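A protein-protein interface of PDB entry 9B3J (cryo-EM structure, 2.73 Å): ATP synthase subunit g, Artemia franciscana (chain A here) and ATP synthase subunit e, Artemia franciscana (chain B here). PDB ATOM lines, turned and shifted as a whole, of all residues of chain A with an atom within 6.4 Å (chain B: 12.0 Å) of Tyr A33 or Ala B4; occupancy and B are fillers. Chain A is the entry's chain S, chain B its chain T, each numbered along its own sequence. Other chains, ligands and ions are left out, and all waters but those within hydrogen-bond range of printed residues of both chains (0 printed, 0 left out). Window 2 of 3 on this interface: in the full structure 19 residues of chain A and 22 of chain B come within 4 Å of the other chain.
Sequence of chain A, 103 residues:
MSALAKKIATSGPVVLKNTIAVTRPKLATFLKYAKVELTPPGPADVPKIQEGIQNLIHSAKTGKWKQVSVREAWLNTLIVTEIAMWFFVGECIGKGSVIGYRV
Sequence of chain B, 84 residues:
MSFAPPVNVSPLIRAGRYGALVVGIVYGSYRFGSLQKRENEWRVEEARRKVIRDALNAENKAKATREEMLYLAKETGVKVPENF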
ATOM      1  N   ALA A  28     -16.988 -30.838  25.458  1.00  0.00           N
ATOM      2  CA  ALA A  28     -16.891 -30.748  24.005  1.00  0.00           C
ATOM      3  C   ALA A  28     -18.180 -30.209  23.398  1.00  0.00           C
ATOM      4  O   ALA A  28     -18.140 -29.461  22.414  1.00  0.00           O
ATOM      5  CB  ALA A  28     -16.550 -32.115  23.415  1.00  0.00           C
ATOM      6  N   THR A  29     -19.330 -30.585  23.964  1.00  0.00           N
ATOM      7  CA  THR A  29     -20.602 -30.049  23.494  1.00  0.00           C
ATOM      8  C   THR A  29     -20.718 -28.561  23.779  1.00  0.00           C
ATOM      9  O   THR A  29     -21.336 -27.832  23.000  1.00  0.00           O
ATOM     10  CB  THR A  29     -21.763 -30.793  24.146  1.00  0.00           C
ATOM     11  OG1 THR A  29     -21.682 -30.647  25.569  1.00  0.00           O
ATOM     12  CG2 THR A  29     -21.714 -32.268  23.792  1.00  0.00           C
ATOM     13  N   PHE A  30     -20.144 -28.096  24.892  1.00  0.00           N
ATOM     14  CA  PHE A  30     -20.083 -26.661  25.150  1.00  0.00           C
ATOM     15  C   PHE A  30     -19.250 -25.951  24.093  1.00  0.00           C
ATOM     16  O   PHE A  30     -19.597 -24.850  23.658  1.00  0.00           O
ATOM     17  CB  PHE A  30     -19.513 -26.399  26.544  1.00  0.00           C
ATOM     18  CG  PHE A  30     -20.549 -26.380  27.635  1.00  0.00           C
ATOM     19  CD1 PHE A  30     -21.869 -26.066  27.355  1.00  0.00           C
ATOM     20  CD2 PHE A  30     -20.198 -26.667  28.946  1.00  0.00           C
ATOM     21  CE1 PHE A  30     -22.819 -26.048  28.359  1.00  0.00           C
ATOM     22  CE2 PHE A  30     -21.144 -26.647  29.953  1.00  0.00           C
ATOM     23  CZ  PHE A  30     -22.454 -26.339  29.658  1.00  0.00           C
ATOM     24  N   LEU A  31     -18.148 -26.573  23.663  1.00  0.00           N
ATOM     25  CA  LEU A  31     -17.357 -26.017  22.569  1.00  0.00           C
ATOM     26  C   LEU A  31     -18.138 -26.031  21.260  1.00  0.00           C
ATOM     27  O   LEU A  31     -18.005 -25.115  20.437  1.00  0.00           O
ATOM     28  CB  LEU A  31     -16.050 -26.797  22.422  1.00  0.00           C
ATOM     29  CG  LEU A  31     -15.128 -26.850  23.641  1.00  0.00           C
ATOM     30  CD1 LEU A  31     -13.871 -27.644  23.324  1.00  0.00           C
ATOM     31  CD2 LEU A  31     -14.770 -25.452  24.114  1.00  0.00           C
ATOM     32  N   LYS A  32     -18.957 -27.065  21.056  1.00  0.00           N
ATOM     33  CA  LYS A  32     -19.812 -27.123  19.876  1.00  0.00           C
ATOM     34  C   LYS A  32     -20.846 -26.004  19.887  1.00  0.00           C
ATOM     35  O   LYS A  32     -21.077 -25.343  18.864  1.00  0.00           O
ATOM     36  CB  LYS A  32     -20.499 -28.484  19.803  1.00  0.00           C
ATOM     37  CG  LYS A  32     -21.561 -28.575  18.731  1.00  0.00           C
ATOM     38  CD  LYS A  32     -22.217 -29.939  18.727  1.00  0.00           C
ATOM     39  CE  LYS A  32     -23.267 -30.036  17.640  1.00  0.00           C
ATOM     40  NZ  LYS A  32     -23.866 -31.394  17.597  1.00  0.00           N
ATOM     41  N   TYR A  33     -21.467 -25.766  21.042  1.00  0.00           N
ATOM     42  CA  TYR A  33     -22.424 -24.673  21.156  1.00  0.00           C
ATOM     43  C   TYR A  33     -21.739 -23.326  21.016  1.00  0.00           C
ATOM     44  O   TYR A  33     -22.336 -22.388  20.489  1.00  0.00           O
ATOM     45  CB  TYR A  33     -23.169 -24.751  22.487  1.00  0.00           C
ATOM     46  CG  TYR A  33     -24.058 -25.961  22.624  1.00  0.00           C
ATOM     47  CD1 TYR A  33     -24.714 -26.490  21.526  1.00  0.00           C
ATOM     48  CD2 TYR A  33     -24.234 -26.578  23.855  1.00  0.00           C
ATOM     49  CE1 TYR A  33     -25.522 -27.596  21.649  1.00  0.00           C
ATOM     50  CE2 TYR A  33     -25.040 -27.686  23.987  1.00  0.00           C
ATOM     51  CZ  TYR A  33     -25.682 -28.189  22.880  1.00  0.00           C
ATOM     52  OH  TYR A  33     -26.489 -29.293  23.004  1.00  0.00           O
ATOM     53  N   ALA A  34     -20.496 -23.212  21.486  1.00  0.00           N
ATOM     54  CA  ALA A  34     -19.747 -21.974  21.319  1.00  0.00           C
ATOM     55  C   ALA A  34     -19.471 -21.696  19.849  1.00  0.00           C
ATOM     56  O   ALA A  34     -19.532 -20.545  19.406  1.00  0.00           O
ATOM     57  CB  ALA A  34     -18.441 -22.043  22.109  1.00  0.00           C
ATOM     58  N   LYS A  35     -19.156 -22.741  19.083  1.00  0.00           N
ATOM     59  CA  LYS A  35     -18.976 -22.574  17.642  1.00  0.00           C
ATOM     60  C   LYS A  35     -20.283 -22.177  16.962  1.00  0.00           C
ATOM     61  O   LYS A  35     -20.288 -21.328  16.061  1.00  0.00           O
ATOM     62  CB  LYS A  35     -18.414 -23.864  17.041  1.00  0.00           C
ATOM     63  CG  LYS A  35     -18.368 -23.906  15.520  1.00  0.00           C
ATOM     64  CD  LYS A  35     -17.489 -22.808  14.936  1.00  0.00           C
ATOM     65  CE  LYS A  35     -16.031 -22.990  15.312  1.00  0.00           C
ATOM     66  NZ  LYS A  35     -15.182 -21.928  14.705  1.00  0.00           N
ATOM     67  N   VAL A  36     -21.398 -22.776  17.381  1.00  0.00           N
ATOM     68  CA  VAL A  36     -22.680 -22.482  16.743  1.00  0.00           C
ATOM     69  C   VAL A  36     -23.178 -21.084  17.111  1.00  0.00           C
ATOM     70  O   VAL A  36     -23.672 -20.344  16.254  1.00  0.00           O
ATOM     71  CB  VAL A  36     -23.707 -23.570  17.106  1.00  0.00           C
ATOM     72  CG1 VAL A  36     -25.093 -23.199  16.608  1.00  0.00           C
ATOM     73  CG2 VAL A  36     -23.284 -24.900  16.514  1.00  0.00           C
ATOM     74  N   GLU A  37     -23.041 -20.690  18.375  1.00  0.00           N
ATOM     75  CA  GLU A  37     -23.743 -19.523  18.893  1.00  0.00           C
ATOM     76  C   GLU A  37     -22.869 -18.306  19.144  1.00  0.00           C
ATOM     77  O   GLU A  37     -23.379 -17.189  19.087  1.00  0.00           O
ATOM     78  CB  GLU A  37     -24.472 -19.882  20.191  1.00  0.00           C
ATOM     79  CG  GLU A  37     -25.614 -20.859  19.981  1.00  0.00           C
ATOM     80  CD  GLU A  37     -26.231 -21.339  21.276  1.00  0.00           C
ATOM     81  OE1 GLU A  37     -25.649 -21.079  22.348  1.00  0.00           O
ATOM     82  OE2 GLU A  37     -27.301 -21.979  21.218  1.00  0.00           O
ATOM     83  N   LEU A  38     -21.576 -18.476  19.415  1.00  0.00           N
ATOM     84  CA  LEU A  38     -20.686 -17.346  19.694  1.00  0.00           C
ATOM     85  C   LEU A  38     -19.859 -16.950  18.478  1.00  0.00           C
ATOM     86  O   LEU A  38     -18.703 -16.545  18.604  1.00  0.00           O
ATOM     87  CB  LEU A  38     -19.776 -17.659  20.877  1.00  0.00           C
ATOM     88  CG  LEU A  38     -20.470 -18.089  22.167  1.00  0.00           C
ATOM     89  CD1 LEU A  38     -19.466 -18.190  23.295  1.00  0.00           C
ATOM     90  CD2 LEU A  38     -21.576 -17.120  22.523  1.00  0.00           C
ATOM     91  N   PHE B   3     -28.021 -31.655  26.653  1.00  0.00           N
ATOM     92  CA  PHE B   3     -28.964 -30.565  26.869  1.00  0.00           C
ATOM     93  C   PHE B   3     -29.949 -30.461  25.712  1.00  0.00           C
ATOM     94  O   PHE B   3     -30.148 -31.411  24.957  1.00  0.00           O
ATOM     95  CB  PHE B   3     -28.229 -29.231  27.040  1.00  0.00           C
ATOM     96  CG  PHE B   3     -27.325 -29.177  28.240  1.00  0.00           C
ATOM     97  CD1 PHE B   3     -27.678 -29.805  29.421  1.00  0.00           C
ATOM     98  CD2 PHE B   3     -26.119 -28.497  28.181  1.00  0.00           C
ATOM     99  CE1 PHE B   3     -26.843 -29.757  30.523  1.00  0.00           C
ATOM    100  CE2 PHE B   3     -25.280 -28.443  29.277  1.00  0.00           C
ATOM    101  CZ  PHE B   3     -25.641 -29.074  30.449  1.00  0.00           C
ATOM    102  N   ALA B   4     -30.559 -29.286  25.590  1.00  0.00           N
ATOM    103  CA  ALA B   4     -31.489 -29.007  24.513  1.00  0.00           C
ATOM    104  C   ALA B   4     -30.733 -28.847  23.195  1.00  0.00           C
ATOM    105  O   ALA B   4     -29.524 -28.605  23.195  1.00  0.00           O
ATOM    106  CB  ALA B   4     -32.286 -27.746  24.840  1.00  0.00           C
ATOM    107  N   PRO B   5     -31.413 -29.021  22.060  1.00  0.00           N
ATOM    108  CA  PRO B   5     -30.765 -28.753  20.778  1.00  0.00           C
ATOM    109  C   PRO B   5     -30.377 -27.293  20.666  1.00  0.00           C
ATOM    110  O   PRO B   5     -31.056 -26.408  21.219  1.00  0.00           O
ATOM    111  CB  PRO B   5     -31.842 -29.131  19.750  1.00  0.00           C
ATOM    112  CG  PRO B   5     -33.120 -29.180  20.516  1.00  0.00           C
ATOM    113  CD  PRO B   5     -32.728 -29.653  21.870  1.00  0.00           C
ATOM    114  N   PRO B   6     -29.275 -26.995  19.979  1.00  0.00           N
ATOM    115  CA  PRO B   6     -28.796 -25.612  19.915  1.00  0.00           C
ATOM    116  C   PRO B   6     -29.720 -24.723  19.105  1.00  0.00           C
ATOM    117  O   PRO B   6     -30.416 -25.170  18.190  1.00  0.00           O
ATOM    118  CB  PRO B   6     -27.429 -25.743  19.239  1.00  0.00           C
ATOM    119  CG  PRO B   6     -27.554 -26.966  18.415  1.00  0.00           C
ATOM    120  CD  PRO B   6     -28.411 -27.907  19.214  1.00  0.00           C
ATOM    121  N   VAL B   7     -29.719 -23.443  19.460  1.00  0.00           N
ATOM    122  CA  VAL B   7     -30.549 -22.436  18.817  1.00  0.00           C
ATOM    123  C   VAL B   7     -29.637 -21.366  18.248  1.00  0.00           C
ATOM    124  O   VAL B   7     -28.777 -20.837  18.960  1.00  0.00           O
ATOM    125  CB  VAL B   7     -31.560 -21.825  19.803  1.00  0.00           C
ATOM    126  CG1 VAL B   7     -32.286 -20.650  19.169  1.00  0.00           C
ATOM    127  CG2 VAL B   7     -32.552 -22.876  20.248  1.00  0.00           C
ATOM    128  N   ASN B   8     -29.812 -21.063  16.965  1.00  0.00           N
ATOM    129  CA  ASN B   8     -29.100 -19.943  16.370  1.00  0.00           C
ATOM    130  C   ASN B   8     -29.657 -18.638  16.919  1.00  0.00           C
ATOM    131  O   ASN B   8     -30.874 -18.425  16.940  1.00  0.00           O
ATOM    132  CB  ASN B   8     -29.216 -19.980  14.848  1.00  0.00           C
ATOM    133  CG  ASN B   8     -30.648 -20.065  14.377  1.00  0.00           C
ATOM    134  OD1 ASN B   8     -31.516 -20.566  15.088  1.00  0.00           O
ATOM    135  ND2 ASN B   8     -30.904 -19.573  13.173  1.00  0.00           N
ATOM    136  N   VAL B   9     -28.759 -17.769  17.380  1.00  0.00           N
ATOM    137  CA  VAL B   9     -29.177 -16.507  17.963  1.00  0.00           C
ATOM    138  C   VAL B   9     -29.728 -15.595  16.871  1.00  0.00           C
ATOM    139  O   VAL B   9     -29.493 -15.795  15.674  1.00  0.00           O
ATOM    140  CB  VAL B   9     -28.000 -15.854  18.705  1.00  0.00           C
ATOM    141  CG1 VAL B   9     -28.485 -15.001  19.856  1.00  0.00           C
ATOM    142  CG2 VAL B   9     -27.055 -16.919  19.220  1.00  0.00           C
ATOM    143  N   SER B  10     -30.505 -14.603  17.293  1.00  0.00           N
ATOM    144  CA  SER B  10     -31.031 -13.626  16.355  1.00  0.00           C
ATOM    145  C   SER B  10     -29.882 -12.828  15.747  1.00  0.00           C
ATOM    146  O   SER B  10     -28.918 -12.498  16.450  1.00  0.00           O
ATOM    147  CB  SER B  10     -32.015 -12.685  17.046  1.00  0.00           C
ATOM    148  OG  SER B  10     -32.462 -11.679  16.155  1.00  0.00           O
ATOM    149  N   ARG B  14     -26.548 -10.940  17.561  1.00  0.00           N
ATOM    150  CA  ARG B  14     -25.149 -11.231  17.266  1.00  0.00           C
ATOM    151  C   ARG B  14     -24.422  -9.999  16.742  1.00  0.00           C
ATOM    152  O   ARG B  14     -23.263  -9.751  17.109  1.00  0.00           O
ATOM    153  CB  ARG B  14     -25.050 -12.375  16.259  1.00  0.00           C
ATOM    154  CG  ARG B  14     -25.022 -13.767  16.866  1.00  0.00           C
ATOM    155  CD  ARG B  14     -24.796 -14.796  15.777  1.00  0.00           C
ATOM    156  NE  ARG B  14     -24.930 -16.168  16.249  1.00  0.00           N
ATOM    157  CZ  ARG B  14     -24.886 -17.231  15.458  1.00  0.00           C
ATOM    158  NH1 ARG B  14     -24.689 -17.116  14.156  1.00  0.00           N
ATOM    159  NH2 ARG B  14     -25.050 -18.439  15.986  1.00  0.00           N
ATOM    160  N   ARG B  17     -23.883  -7.606  19.635  1.00  0.00           N
ATOM    161  CA  ARG B  17     -22.923  -8.149  20.590  1.00  0.00           C
ATOM    162  C   ARG B  17     -21.497  -7.999  20.087  1.00  0.00           C
ATOM    163  O   ARG B  17     -20.612  -7.544  20.822  1.00  0.00           O
ATOM    164  CB  ARG B  17     -23.241  -9.614  20.854  1.00  0.00           C
ATOM    165  CG  ARG B  17     -22.180 -10.343  21.630  1.00  0.00           C
ATOM    166  CD  ARG B  17     -22.425 -11.841  21.612  1.00  0.00           C
ATOM    167  NE  ARG B  17     -23.623 -12.228  22.350  1.00  0.00           N
ATOM    168  CZ  ARG B  17     -24.779 -12.552  21.788  1.00  0.00           C
ATOM    169  NH1 ARG B  17     -24.940 -12.528  20.477  1.00  0.00           N
ATOM    170  NH2 ARG B  17     -25.798 -12.910  22.563  1.00  0.00           N
ATOM    171  N   TYR B  18     -21.251  -8.364  18.827  1.00  0.00           N
ATOM    172  CA  TYR B  18     -19.905  -8.214  18.291  1.00  0.00           C
ATOM    173  C   TYR B  18     -19.571  -6.765  17.975  1.00  0.00           C
ATOM    174  O   TYR B  18     -18.396  -6.381  18.039  1.00  0.00           O
ATOM    175  CB  TYR B  18     -19.729  -9.086  17.057  1.00  0.00           C
ATOM    176  CG  TYR B  18     -19.274 -10.474  17.407  1.00  0.00           C
ATOM    177  CD1 TYR B  18     -17.951 -10.722  17.739  1.00  0.00           C
ATOM    178  CD2 TYR B  18     -20.163 -11.531  17.427  1.00  0.00           C
ATOM    179  CE1 TYR B  18     -17.524 -11.988  18.068  1.00  0.00           C
ATOM    180  CE2 TYR B  18     -19.746 -12.801  17.755  1.00  0.00           C
ATOM    181  CZ  TYR B  18     -18.425 -13.023  18.074  1.00  0.00           C
ATOM    182  OH  TYR B  18     -18.008 -14.291  18.401  1.00  0.00           O
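OE2 of Glu A37 lies within hydrogen-bond range of N of Val B7. NH2 of Arg B14 lies close to O of Val A36, at 2.4 Å. OH of Tyr A33 sits at hydrogen-bond distance from O of Ala B4 (3.1 Å). The backbone carbonyl oxygen (O) of Glu A37 sits at hydrogen-bond distance from the guanidinium group (NE) of Arg B14, at 3.4 Å. The backbone carbonyl oxygen (O) of Leu A38 lies close to the side-chain hydroxyl (OH) of Tyr B18.
Among the printed residues, pairs that only touch across the chains: Phe A30 with Phe B3 (3.5 Å), Tyr A33 with Pro B6 (3.6 Å) and Glu A37 with Val B9 (3.7 Å).
No residue of chain B comes within 4 Å of Lys A32. No residue of chain B comes within 4 Å of Ala A34. Printed residues of chain B within 4 Å of Val A36: Arg B14 (2.4 Å). Of the printed residues of chain B, Leu A38 touches Tyr B18 (2.4 Å). Of the printed residues of chain A, Phe B3 touches Phe A30 (3.5 Å). Ala B4 touches one residue of chain A. Ser B10 touches none of the printed residues of chain A. Arg B17 touches none of the printed residues of chain A. Printed residues of chain A within 4 Å of Tyr B18: Leu A38. The nearest residue of chain B that does not touch Tyr A33 is Phe B3 (4.4 Å).
Of the 11 printed residues of chain B, 7 touch a printed residue of chain A. Printed residues of chain B that touch a printed residue of chain A: Phe B3, Ala B4, Pro B6, Val B7, Val B9, Arg B14 and Tyr B18. Hydrophobic or aromatic side chains of chain B that line the printed part of chain A: Phe B3, Pro B6, Val B9 and Tyr B18. Along chain B the printed residues that touch a printed residue of chain A span positions 3 to 18. Among the printed residues, no Asp or Glu carboxylate lies within 4 Å of a Lys or Arg side-chain nitrogen of the other chain.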
